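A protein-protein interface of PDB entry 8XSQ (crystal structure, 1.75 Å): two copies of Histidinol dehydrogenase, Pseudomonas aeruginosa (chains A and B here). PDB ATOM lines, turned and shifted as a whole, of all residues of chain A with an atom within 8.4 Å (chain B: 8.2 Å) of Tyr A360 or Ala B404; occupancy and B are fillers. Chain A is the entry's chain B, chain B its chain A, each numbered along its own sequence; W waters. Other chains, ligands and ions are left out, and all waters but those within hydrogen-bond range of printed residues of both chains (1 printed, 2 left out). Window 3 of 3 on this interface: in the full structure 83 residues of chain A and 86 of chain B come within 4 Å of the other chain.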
ATOM      1  N   THR A 253      -2.846  -0.189  10.062  1.00  0.00           N
ATOM      2  CA  THR A 253      -1.404  -0.043   9.915  1.00  0.00           C
ATOM      3  C   THR A 253      -0.767   0.014  11.297  1.00  0.00           C
ATOM      4  O   THR A 253      -1.360   0.546  12.239  1.00  0.00           O
ATOM      5  CB  THR A 253      -1.052   1.217   9.118  1.00  0.00           C
ATOM      6  OG1 THR A 253      -1.714   1.176   7.848  1.00  0.00           O
ATOM      7  CG2 THR A 253       0.453   1.316   8.882  1.00  0.00           C
ATOM      8  N   TRP A 257       4.638   2.589  12.739  1.00  0.00           N
ATOM      9  CA  TRP A 257       4.868   3.039  11.368  1.00  0.00           C
ATOM     10  C   TRP A 257       4.228   4.402  11.133  1.00  0.00           C
ATOM     11  O   TRP A 257       4.857   5.314  10.583  1.00  0.00           O
ATOM     12  CB  TRP A 257       4.308   2.026  10.364  1.00  0.00           C
ATOM     13  CG  TRP A 257       4.934   0.660  10.379  1.00  0.00           C
ATOM     14  CD1 TRP A 257       5.717   0.116  11.356  1.00  0.00           C
ATOM     15  CD2 TRP A 257       4.815  -0.338   9.356  1.00  0.00           C
ATOM     16  NE1 TRP A 257       6.091  -1.162  11.005  1.00  0.00           N
ATOM     17  CE2 TRP A 257       5.552  -1.462   9.782  1.00  0.00           C
ATOM     18  CE3 TRP A 257       4.155  -0.390   8.123  1.00  0.00           C
ATOM     19  CZ2 TRP A 257       5.649  -2.624   9.017  1.00  0.00           C
ATOM     20  CZ3 TRP A 257       4.251  -1.544   7.365  1.00  0.00           C
ATOM     21  CH2 TRP A 257       4.993  -2.646   7.814  1.00  0.00           C
ATOM     22  N   ASP A 261       5.941   7.880  10.250  1.00  0.00           N
ATOM     23  CA  ASP A 261       5.573   8.597   9.033  1.00  0.00           C
ATOM     24  C   ASP A 261       5.247  10.054   9.335  1.00  0.00           C
ATOM     25  O   ASP A 261       5.587  10.950   8.555  1.00  0.00           O
ATOM     26  CB  ASP A 261       4.391   7.908   8.352  1.00  0.00           C
ATOM     27  CG  ASP A 261       4.756   6.551   7.789  1.00  0.00           C
ATOM     28  OD1 ASP A 261       5.962   6.269   7.648  1.00  0.00           O
ATOM     29  OD2 ASP A 261       3.840   5.758   7.505  1.00  0.00           O
ATOM     30  N   GLU A 336      -0.844  10.365   2.417  1.00  0.00           N
ATOM     31  CA  GLU A 336      -0.528   8.963   2.671  1.00  0.00           C
ATOM     32  C   GLU A 336      -1.835   8.235   2.972  1.00  0.00           C
ATOM     33  O   GLU A 336      -2.407   8.382   4.055  1.00  0.00           O
ATOM     34  CB  GLU A 336       0.469   8.817   3.814  1.00  0.00           C
ATOM     35  CG  GLU A 336       0.809   7.370   4.120  1.00  0.00           C
ATOM     36  CD  GLU A 336       1.880   7.217   5.181  1.00  0.00           C
ATOM     37  OE1 GLU A 336       2.848   8.003   5.185  1.00  0.00           O
ATOM     38  OE2 GLU A 336       1.757   6.295   6.009  1.00  0.00           O
ATOM     39  N   LEU A 337      -2.313   7.453   2.002  1.00  0.00           N
ATOM     40  CA  LEU A 337      -3.566   6.713   2.142  1.00  0.00           C
ATOM     41  C   LEU A 337      -3.243   5.334   2.714  1.00  0.00           C
ATOM     42  O   LEU A 337      -3.208   4.320   2.013  1.00  0.00           O
ATOM     43  CB  LEU A 337      -4.283   6.616   0.801  1.00  0.00           C
ATOM     44  CG  LEU A 337      -5.485   7.529   0.563  1.00  0.00           C
ATOM     45  CD1 LEU A 337      -6.070   7.289  -0.826  1.00  0.00           C
ATOM     46  CD2 LEU A 337      -6.550   7.347   1.638  1.00  0.00           C
ATOM     47  N   SER A 338      -3.003   5.308   4.024  1.00  0.00           N
ATOM     48  CA  SER A 338      -2.596   4.081   4.711  1.00  0.00           C
ATOM     49  C   SER A 338      -3.838   3.284   5.110  1.00  0.00           C
ATOM     50  O   SER A 338      -4.238   3.216   6.273  1.00  0.00           O
ATOM     51  CB  SER A 338      -1.726   4.414   5.917  1.00  0.00           C
ATOM     52  OG  SER A 338      -1.038   3.269   6.384  1.00  0.00           O
ATOM     53  N   VAL A 339      -4.460   2.673   4.102  1.00  0.00           N
ATOM     54  CA  VAL A 339      -5.683   1.903   4.280  1.00  0.00           C
ATOM     55  C   VAL A 339      -5.570   0.603   3.492  1.00  0.00           C
ATOM     56  O   VAL A 339      -4.688   0.432   2.647  1.00  0.00           O
ATOM     57  CB  VAL A 339      -6.940   2.692   3.848  1.00  0.00           C
ATOM     58  CG1 VAL A 339      -7.023   4.024   4.582  1.00  0.00           C
ATOM     59  CG2 VAL A 339      -6.931   2.922   2.356  1.00  0.00           C
ATOM     60  N   PHE A 356       0.506   8.518  -1.632  1.00  0.00           N
ATOM     61  CA  PHE A 356       1.223   7.312  -1.240  1.00  0.00           C
ATOM     62  C   PHE A 356       0.194   6.329  -0.700  1.00  0.00           C
ATOM     63  O   PHE A 356      -0.516   6.640   0.263  1.00  0.00           O
ATOM     64  CB  PHE A 356       2.287   7.648  -0.197  1.00  0.00           C
ATOM     65  CG  PHE A 356       3.173   8.794  -0.599  1.00  0.00           C
ATOM     66  CD1 PHE A 356       4.247   8.592  -1.444  1.00  0.00           C
ATOM     67  CD2 PHE A 356       2.895  10.084  -0.180  1.00  0.00           C
ATOM     68  CE1 PHE A 356       5.052   9.643  -1.838  1.00  0.00           C
ATOM     69  CE2 PHE A 356       3.695  11.144  -0.573  1.00  0.00           C
ATOM     70  CZ  PHE A 356       4.777  10.921  -1.402  1.00  0.00           C
ATOM     71  N   MET A 357       0.096   5.162  -1.329  1.00  0.00           N
ATOM     72  CA  MET A 357      -1.022   4.255  -1.112  1.00  0.00           C
ATOM     73  C   MET A 357      -0.588   3.007  -0.361  1.00  0.00           C
ATOM     74  O   MET A 357       0.460   2.423  -0.656  1.00  0.00           O
ATOM     75  CB  MET A 357      -1.654   3.833  -2.441  1.00  0.00           C
ATOM     76  CG  MET A 357      -2.522   4.882  -3.107  1.00  0.00           C
ATOM     77  SD  MET A 357      -3.460   4.115  -4.437  1.00  0.00           S
ATOM     78  CE  MET A 357      -4.646   5.398  -4.817  1.00  0.00           C
ATOM     79  N   GLY A 358      -1.420   2.583   0.585  1.00  0.00           N
ATOM     80  CA  GLY A 358      -1.202   1.330   1.274  1.00  0.00           C
ATOM     81  C   GLY A 358      -0.260   1.472   2.448  1.00  0.00           C
ATOM     82  O   GLY A 358       0.315   2.526   2.715  1.00  0.00           O
ATOM     83  N   ARG A 359      -0.096   0.363   3.166  1.00  0.00           N
ATOM     84  CA  ARG A 359       0.686   0.375   4.392  1.00  0.00           C
ATOM     85  C   ARG A 359       2.186   0.313   4.144  1.00  0.00           C
ATOM     86  O   ARG A 359       2.960   0.600   5.063  1.00  0.00           O
ATOM     87  CB  ARG A 359       0.256  -0.789   5.282  1.00  0.00           C
ATOM     88  CG  ARG A 359      -1.251  -0.859   5.433  1.00  0.00           C
ATOM     89  CD  ARG A 359      -1.704  -2.116   6.152  1.00  0.00           C
ATOM     90  NE  ARG A 359      -3.133  -2.386   5.998  1.00  0.00           N
ATOM     91  CZ  ARG A 359      -4.118  -1.543   6.284  1.00  0.00           C
ATOM     92  NH1 ARG A 359      -3.890  -0.339   6.789  1.00  0.00           N
ATOM     93  NH2 ARG A 359      -5.373  -1.929   6.086  1.00  0.00           N
ATOM     94  N   TYR A 360       2.613  -0.039   2.933  1.00  0.00           N
ATOM     95  CA  TYR A 360       4.029  -0.202   2.625  1.00  0.00           C
ATOM     96  C   TYR A 360       4.653   1.026   1.978  1.00  0.00           C
ATOM     97  O   TYR A 360       5.835   0.985   1.626  1.00  0.00           O
ATOM     98  CB  TYR A 360       4.234  -1.416   1.711  1.00  0.00           C
ATOM     99  CG  TYR A 360       3.692  -2.703   2.280  1.00  0.00           C
ATOM    100  CD1 TYR A 360       4.206  -3.234   3.453  1.00  0.00           C
ATOM    101  CD2 TYR A 360       2.660  -3.385   1.646  1.00  0.00           C
ATOM    102  CE1 TYR A 360       3.713  -4.410   3.981  1.00  0.00           C
ATOM    103  CE2 TYR A 360       2.159  -4.562   2.167  1.00  0.00           C
ATOM    104  CZ  TYR A 360       2.688  -5.069   3.335  1.00  0.00           C
ATOM    105  OH  TYR A 360       2.192  -6.241   3.858  1.00  0.00           O
ATOM    106  N   THR A 361       3.907   2.114   1.815  1.00  0.00           N
ATOM    107  CA  THR A 361       4.409   3.293   1.119  1.00  0.00           C
ATOM    108  C   THR A 361       4.382   4.487   2.063  1.00  0.00           C
ATOM    109  O   THR A 361       3.312   5.011   2.388  1.00  0.00           O
ATOM    110  CB  THR A 361       3.594   3.576  -0.139  1.00  0.00           C
ATOM    111  OG1 THR A 361       3.457   2.367  -0.897  1.00  0.00           O
ATOM    112  CG2 THR A 361       4.300   4.617  -0.994  1.00  0.00           C
ATOM    113  N   ALA A 362       5.561   4.911   2.499  1.00  0.00           N
ATOM    114  CA  ALA A 362       5.720   6.122   3.285  1.00  0.00           C
ATOM    115  C   ALA A 362       6.161   7.263   2.378  1.00  0.00           C
ATOM    116  O   ALA A 362       6.865   7.051   1.387  1.00  0.00           O
ATOM    117  CB  ALA A 362       6.745   5.909   4.397  1.00  0.00           C
ATOM    118  N   GLU A 363       5.740   8.483   2.724  1.00  0.00           N
ATOM    119  CA  GLU A 363       6.134   9.639   1.926  1.00  0.00           C
ATOM    120  C   GLU A 363       7.633   9.893   1.987  1.00  0.00           C
ATOM    121  O   GLU A 363       8.155  10.628   1.143  1.00  0.00           O
ATOM    122  CB  GLU A 363       5.382  10.893   2.373  1.00  0.00           C
ATOM    123  CG  GLU A 363       5.900  11.498   3.658  1.00  0.00           C
ATOM    124  CD  GLU A 363       5.335  10.806   4.873  1.00  0.00           C
ATOM    125  OE1 GLU A 363       4.195  10.299   4.788  1.00  0.00           O
ATOM    126  OE2 GLU A 363       6.036  10.754   5.903  1.00  0.00           O
ATOM    127  N   LEU A 365       9.663   7.759   1.109  1.00  0.00           N
ATOM    128  CA  LEU A 365      10.049   7.255  -0.203  1.00  0.00           C
ATOM    129  C   LEU A 365       9.854   8.311  -1.284  1.00  0.00           C
ATOM    130  O   LEU A 365      10.638   8.369  -2.238  1.00  0.00           O
ATOM    131  CB  LEU A 365       9.253   5.996  -0.541  1.00  0.00           C
ATOM    132  CG  LEU A 365       9.438   4.824   0.423  1.00  0.00           C
ATOM    133  CD1 LEU A 365       8.731   3.583  -0.103  1.00  0.00           C
ATOM    134  CD2 LEU A 365      10.917   4.552   0.653  1.00  0.00           C
ATOM    135  N   ASP B 119       7.599  -6.538  -9.237  1.00  0.00           N
ATOM    136  CA  ASP B 119       7.544  -6.839  -7.812  1.00  0.00           C
ATOM    137  C   ASP B 119       6.187  -6.521  -7.188  1.00  0.00           C
ATOM    138  O   ASP B 119       6.038  -6.633  -5.968  1.00  0.00           O
ATOM    139  CB  ASP B 119       8.669  -6.108  -7.061  1.00  0.00           C
ATOM    140  CG  ASP B 119       8.552  -4.587  -7.119  1.00  0.00           C
ATOM    141  OD1 ASP B 119       7.458  -4.051  -7.386  1.00  0.00           O
ATOM    142  OD2 ASP B 119       9.579  -3.917  -6.877  1.00  0.00           O
ATOM    143  N   GLY B 120       5.200  -6.132  -7.994  1.00  0.00           N
ATOM    144  CA  GLY B 120       3.872  -5.857  -7.495  1.00  0.00           C
ATOM    145  C   GLY B 120       3.584  -4.403  -7.192  1.00  0.00           C
ATOM    146  O   GLY B 120       2.415  -4.056  -6.975  1.00  0.00           O
ATOM    147  N   THR B 121       4.605  -3.548  -7.161  1.00  0.00           N
ATOM    148  CA  THR B 121       4.383  -2.125  -6.943  1.00  0.00           C
ATOM    149  C   THR B 121       3.563  -1.541  -8.084  1.00  0.00           C
ATOM    150  O   THR B 121       3.815  -1.820  -9.260  1.00  0.00           O
ATOM    151  CB  THR B 121       5.722  -1.389  -6.831  1.00  0.00           C
ATOM    152  OG1 THR B 121       6.409  -1.819  -5.649  1.00  0.00           O
ATOM    153  CG2 THR B 121       5.504   0.113  -6.754  1.00  0.00           C
ATOM    154  N   ILE B 400       1.938   6.166  -5.902  1.00  0.00           N
ATOM    155  CA  ILE B 400       2.879   5.074  -5.680  1.00  0.00           C
ATOM    156  C   ILE B 400       2.282   4.155  -4.624  1.00  0.00           C
ATOM    157  O   ILE B 400       1.939   4.604  -3.524  1.00  0.00           O
ATOM    158  CB  ILE B 400       4.271   5.578  -5.258  1.00  0.00           C
ATOM    159  CG1 ILE B 400       5.156   4.412  -4.816  1.00  0.00           C
ATOM    160  CG2 ILE B 400       4.166   6.622  -4.174  1.00  0.00           C
ATOM    161  CD1 ILE B 400       6.633   4.700  -4.930  1.00  0.00           C
ATOM    162  N   ASN B 401       2.137   2.877  -4.964  1.00  0.00           N
ATOM    163  CA  ASN B 401       1.499   1.893  -4.095  1.00  0.00           C
ATOM    164  C   ASN B 401       2.463   0.711  -4.051  1.00  0.00           C
ATOM    165  O   ASN B 401       2.344  -0.229  -4.842  1.00  0.00           O
ATOM    166  CB  ASN B 401       0.114   1.504  -4.624  1.00  0.00           C
ATOM    167  CG  ASN B 401      -0.608   0.525  -3.720  1.00  0.00           C
ATOM    168  OD1 ASN B 401      -0.048   0.031  -2.740  1.00  0.00           O
ATOM    169  ND2 ASN B 401      -1.865   0.231  -4.052  1.00  0.00           N
ATOM    170  N   CYS B 402       3.427   0.776  -3.139  1.00  0.00           N
ATOM    171  CA  CYS B 402       4.463  -0.242  -3.070  1.00  0.00           C
ATOM    172  C   CYS B 402       3.901  -1.568  -2.581  1.00  0.00           C
ATOM    173  O   CYS B 402       3.059  -1.613  -1.679  1.00  0.00           O
ATOM    174  CB  CYS B 402       5.590   0.197  -2.132  1.00  0.00           C
ATOM    175  SG  CYS B 402       6.629   1.533  -2.740  1.00  0.00           S
ATOM    176  N   SER B 403       4.370  -2.651  -3.189  1.00  0.00           N
ATOM    177  CA  SER B 403       4.303  -3.947  -2.541  1.00  0.00           C
ATOM    178  C   SER B 403       5.356  -4.004  -1.436  1.00  0.00           C
ATOM    179  O   SER B 403       6.187  -3.104  -1.288  1.00  0.00           O
ATOM    180  CB  SER B 403       4.530  -5.067  -3.554  1.00  0.00           C
ATOM    181  OG  SER B 403       5.820  -4.959  -4.133  1.00  0.00           O
ATOM    182  N   ALA B 404       5.315  -5.076  -0.642  1.00  0.00           N
ATOM    183  CA  ALA B 404       6.326  -5.238   0.398  1.00  0.00           C
ATOM    184  C   ALA B 404       7.722  -5.324  -0.207  1.00  0.00           C
ATOM    185  O   ALA B 404       8.675  -4.737   0.319  1.00  0.00           O
ATOM    186  CB  ALA B 404       6.023  -6.479   1.239  1.00  0.00           C
ATOM    187  N   GLU B 405       7.855  -6.035  -1.331  1.00  0.00           N
ATOM    188  CA  GLU B 405       9.152  -6.149  -1.991  1.00  0.00           C
ATOM    189  C   GLU B 405       9.580  -4.824  -2.612  1.00  0.00           C
ATOM    190  O   GLU B 405      10.755  -4.448  -2.533  1.00  0.00           O
ATOM    191  CB  GLU B 405       9.095  -7.259  -3.043  1.00  0.00           C
ATOM    192  CG  GLU B 405      10.288  -7.316  -3.978  1.00  0.00           C
ATOM    193  CD  GLU B 405      10.231  -8.503  -4.926  1.00  0.00           C
ATOM    194  OE1 GLU B 405       9.121  -9.028  -5.170  1.00  0.00           O
ATOM    195  OE2 GLU B 405      11.299  -8.912  -5.427  1.00  0.00           O
ATOM    196  N   GLY B 406       8.644  -4.098  -3.229  1.00  0.00           N
ATOM    197  CA  GLY B 406       8.994  -2.815  -3.819  1.00  0.00           C
ATOM    198  C   GLY B 406       9.405  -1.788  -2.780  1.00  0.00           C
ATOM    199  O   GLY B 406      10.333  -1.005  -3.000  1.00  0.00           O
ATOM    200  N   ALA B 407       8.725  -1.781  -1.630  1.00  0.00           N
ATOM    201  CA  ALA B 407       9.111  -0.879  -0.553  1.00  0.00           C
ATOM    202  C   ALA B 407      10.484  -1.229   0.008  1.00  0.00           C
ATOM    203  O   ALA B 407      11.174  -0.353   0.543  1.00  0.00           O
ATOM    204  CB  ALA B 407       8.064  -0.906   0.557  1.00  0.00           C
ATOM    205  N   SER B 408      10.891  -2.496  -0.093  1.00  0.00           N
ATOM    206  CA  SER B 408      12.227  -2.878   0.353  1.00  0.00           C
ATOM    207  C   SER B 408      13.294  -2.360  -0.600  1.00  0.00           C
ATOM    208  O   SER B 408      14.346  -1.879  -0.161  1.00  0.00           O
ATOM    209  CB  SER B 408      12.326  -4.396   0.485  1.00  0.00           C
ATOM    210  OG  SER B 408      11.273  -4.897   1.280  1.00  0.00           O
ATOM    211  N   VAL B 409      13.047  -2.464  -1.907  1.00  0.00           N
ATOM    212  CA  VAL B 409      13.995  -1.944  -2.889  1.00  0.00           C
ATOM    213  C   VAL B 409      14.169  -0.442  -2.706  1.00  0.00           C
ATOM    214  O   VAL B 409      15.290   0.065  -2.581  1.00  0.00           O
ATOM    215  CB  VAL B 409      13.531  -2.285  -4.316  1.00  0.00           C
ATOM    216  CG1 VAL B 409      14.405  -1.575  -5.344  1.00  0.00           C
ATOM    217  CG2 VAL B 409      13.547  -3.788  -4.535  1.00  0.00           C
ATOM    218  N   LEU B 410      13.056   0.292  -2.681  1.00  0.00           N
ATOM    219  CA  LEU B 410      13.129   1.737  -2.504  1.00  0.00           C
ATOM    220  C   LEU B 410      13.639   2.101  -1.115  1.00  0.00           C
ATOM    221  O   LEU B 410      14.383   3.075  -0.957  1.00  0.00           O
ATOM    222  CB  LEU B 410      11.756   2.363  -2.752  1.00  0.00           C
ATOM    223  CG  LEU B 410      11.191   2.168  -4.161  1.00  0.00           C
ATOM    224  CD1 LEU B 410       9.826   2.822  -4.282  1.00  0.00           C
ATOM    225  CD2 LEU B 410      12.151   2.722  -5.201  1.00  0.00           C
ATOM    226  N   GLY B 411      13.253   1.326  -0.098  1.00  0.00           N
ATOM    227  CA  GLY B 411      13.626   1.665   1.264  1.00  0.00           C
ATOM    228  C   GLY B 411      15.111   1.544   1.527  1.00  0.00           C
ATOM    229  O   GLY B 411      15.670   2.314   2.313  1.00  0.00           O
ATOM    230  N   SER B 429      11.235   5.371   8.994  1.00  0.00           N
ATOM    231  CA  SER B 429       9.951   5.188   8.327  1.00  0.00           C
ATOM    232  C   SER B 429      10.092   4.267   7.122  1.00  0.00           C
ATOM    233  O   SER B 429       9.234   3.410   6.879  1.00  0.00           O
ATOM    234  CB  SER B 429       9.381   6.547   7.922  1.00  0.00           C
ATOM    235  OG  SER B 429       8.642   6.464   6.725  1.00  0.00           O
ATOM    236  N   ALA B 430      11.184   4.412   6.367  1.00  0.00           N
ATOM    237  CA  ALA B 430      11.425   3.509   5.248  1.00  0.00           C
ATOM    238  C   ALA B 430      11.865   2.133   5.733  1.00  0.00           C
ATOM    239  O   ALA B 430      11.486   1.112   5.145  1.00  0.00           O
ATOM    240  CB  ALA B 430      12.470   4.106   4.306  1.00  0.00           C
ATOM    241  N   TYR B 432      11.015   0.442   8.323  1.00  0.00           N
ATOM    242  CA  TYR B 432       9.925  -0.402   8.802  1.00  0.00           C
ATOM    243  C   TYR B 432       9.439  -1.357   7.721  1.00  0.00           C
ATOM    244  O   TYR B 432       8.948  -2.449   8.028  1.00  0.00           O
ATOM    245  CB  TYR B 432       8.759   0.462   9.286  1.00  0.00           C
ATOM    246  CG  TYR B 432       8.881   0.949  10.712  1.00  0.00           C
ATOM    247  CD1 TYR B 432       9.174   0.067  11.745  1.00  0.00           C
ATOM    248  CD2 TYR B 432       8.695   2.289  11.025  1.00  0.00           C
ATOM    249  CE1 TYR B 432       9.280   0.508  13.052  1.00  0.00           C
ATOM    250  CE2 TYR B 432       8.800   2.740  12.327  1.00  0.00           C
ATOM    251  CZ  TYR B 432       9.092   1.847  13.336  1.00  0.00           C
ATOM    252  OH  TYR B 432       9.200   2.293  14.635  1.00  0.00           O
ATOM    253  N   ARG B 433       9.573  -0.967   6.456  1.00  0.00           N
ATOM    254  CA  ARG B 433       9.033  -1.723   5.336  1.00  0.00           C
ATOM    255  C   ARG B 433      10.079  -2.568   4.620  1.00  0.00           C
ATOM    256  O   ARG B 433       9.736  -3.269   3.663  1.00  0.00           O
ATOM    257  CB  ARG B 433       8.364  -0.769   4.342  1.00  0.00           C
ATOM    258  CG  ARG B 433       6.963  -0.322   4.752  1.00  0.00           C
ATOM    259  CD  ARG B 433       6.978   0.843   5.740  1.00  0.00           C
ATOM    260  NE  ARG B 433       5.679   1.504   5.811  1.00  0.00           N
ATOM    261  CZ  ARG B 433       5.447   2.655   6.429  1.00  0.00           C
ATOM    262  NH1 ARG B 433       6.411   3.311   7.056  1.00  0.00           N
ATOM    263  NH2 ARG B 433       4.216   3.157   6.423  1.00  0.00           N
ATOM    264  N   ILE B 434      11.336  -2.523   5.051  1.00  0.00           N
ATOM    265  CA  ILE B 434      12.388  -3.309   4.414  1.00  0.00           C
ATOM    266  C   ILE B 434      12.332  -4.740   4.933  1.00  0.00           C
ATOM    267  O   ILE B 434      12.316  -4.975   6.147  1.00  0.00           O
ATOM    268  CB  ILE B 434      13.769  -2.685   4.668  1.00  0.00           C
ATOM    269  CG1 ILE B 434      13.857  -1.294   4.036  1.00  0.00           C
ATOM    270  CG2 ILE B 434      14.872  -3.588   4.135  1.00  0.00           C
ATOM    271  CD1 ILE B 434      15.113  -0.538   4.410  1.00  0.00           C
ATOM    272  N   LEU B 435      12.303  -5.700   4.010  1.00  0.00           N
ATOM    273  CA  LEU B 435      12.372  -7.112   4.357  1.00  0.00           C
ATOM    274  C   LEU B 435      13.820  -7.584   4.364  1.00  0.00           C
ATOM    275  O   LEU B 435      14.631  -7.158   3.537  1.00  0.00           O
ATOM    276  CB  LEU B 435      11.561  -7.959   3.375  1.00  0.00           C
ATOM    277  CG  LEU B 435      10.253  -7.375   2.843  1.00  0.00           C
ATOM    278  CD1 LEU B 435       9.832  -8.076   1.558  1.00  0.00           C
ATOM    279  CD2 LEU B 435       9.161  -7.483   3.892  1.00  0.00           C
HETATM  280  O   HOH W   1       7.615   8.741   5.719  1.00  0.00           O
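Hydrophobic or aromatic side chains of chain A within 4 Å of the printed part of chain B: Trp A257, Phe A356, Met A357, Tyr A360, Ala A362 and Leu A365. Along chain A the printed residues that touch a printed residue of chain B span positions 257 to 365. Of the 21 printed residues of chain B, 10 touch a printed residue of chain A. Printed residues of chain B that touch a printed residue of chain A: Ile B400, Asn B401, Cys B402, Ser B403, Ala B404, Ala B407, Ser B429, Ala B430, Tyr B432 and Arg B433. Hydrophobic or aromatic side chains of chain B within 4 Å of the printed part of chain A: Ile B400, Ala B407, Ala B430 and Tyr B432. Among the printed residues, 20 pairs touch across the chains. Among the printed residues, Asp or Glu carboxylates within 4 Å of a Lys or Arg side-chain nitrogen of the other chain: Asp A261 with Arg B433 (2.8 Å).
Tyr B432 touches Trp A257. Arg B433 touches Trp A257 (NE to CE3, 3.4 Å). CD1 of Phe A356 touches CG2 of Ile B400, at 3.4 Å. O of Ser B403 touches CB of Tyr A360, at 3.96 Å. O of Ile B400 touches CG2 of Thr A361, 3.5 Å away. C of Asn B401 touches OG1 of Thr A361, 3.7 Å away. Ala A362 touches Ser B429 (CB to OG, 3.1 Å). Arg B433 touches Ala A362. Leu A365 touches Cys B402. Leu A365 touches Ala B430.
No position is printed for both chains. Of the 20 pairs that touch across the chains among the printed residues, none has its exchanged pair printed and touching as well.
Of chain B, only Cys B402, Ser B403, Ala B404, Ala B407 and Arg B433 come within 4 Å of Tyr A360. Ala B404 touches just one residue of chain A: Tyr A360. Of chain A, only Tyr A360 comes within 4 Å of Ser B403. Printed residues of chain B within 4 Å of Asp A261: Ser B429 and Arg B433. Of the printed residues of chain A, Ile B400 touches Phe A356, Met A357 and Thr A361. Printed residues of chain A within 4 Å of Ala B407: Tyr A360 (3.1 Å). Of the printed residues of chain B, Leu A365 touches Cys B402 (3.9 Å) and Ala B430 (3.99 Å). Gly B406 touches none of the printed residues of chain A. The nearest printed residue of chain A that does not touch Ala B407 is Leu A365 (4.5 Å).
The backbone carbonyl oxygen (O) of Asp B119 is in hydrogen-bond range of the side-chain hydroxyl (OG) of Ser B403 (2.5 Å). The backbone NH (N) of Ser B403 is in hydrogen-bond range of the side-chain hydroxyl (OG1) of Thr B121, 3.3 Å away. The side-chain hydroxyl (OG) of Ser B403 lies within hydrogen-bond range of the backbone NH (N) of Gly B406 (3.1 Å). O of Ser B429 is in hydrogen-bond range of NH1 of Arg B433, 2.8 Å away. The side-chain hydroxyl of Thr A253 lies within hydrogen-bond range of the guanidinium group of Arg A359 (2.9 Å). The side-chain carboxylate of Asp A261 sits close to the side-chain carboxylate of Glu A336 (2.6 Å).
Water W1 bridges OE2 of Glu A363 (2.6 Å) and OG of Ser B429 (2.7 Å).
The backbone NH (N) of Met A357 lies within hydrogen-bond range of the backbone carbonyl oxygen (O) of Ile B400 (2.9 Å). O of Met A357 sits close to OD1 of Asn B401 (3.2 Å). The backbone NH (N) of Cys B402 lies within hydrogen-bond range of the side-chain hydroxyl (OG1) of Thr A361 (2.7 Å). The side-chain hydroxyl (OG) of Ser B429 lies within hydrogen-bond range of the side-chain carboxylate (OD1) of Asp A261 (2.8 Å). The guanidinium group of Arg B433 is in salt-bridge range of the side-chain carboxylate of Asp A261 (2.8 Å). O of Arg A359 is in hydrogen-bond range of NE of Arg B433 (3.0 Å).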
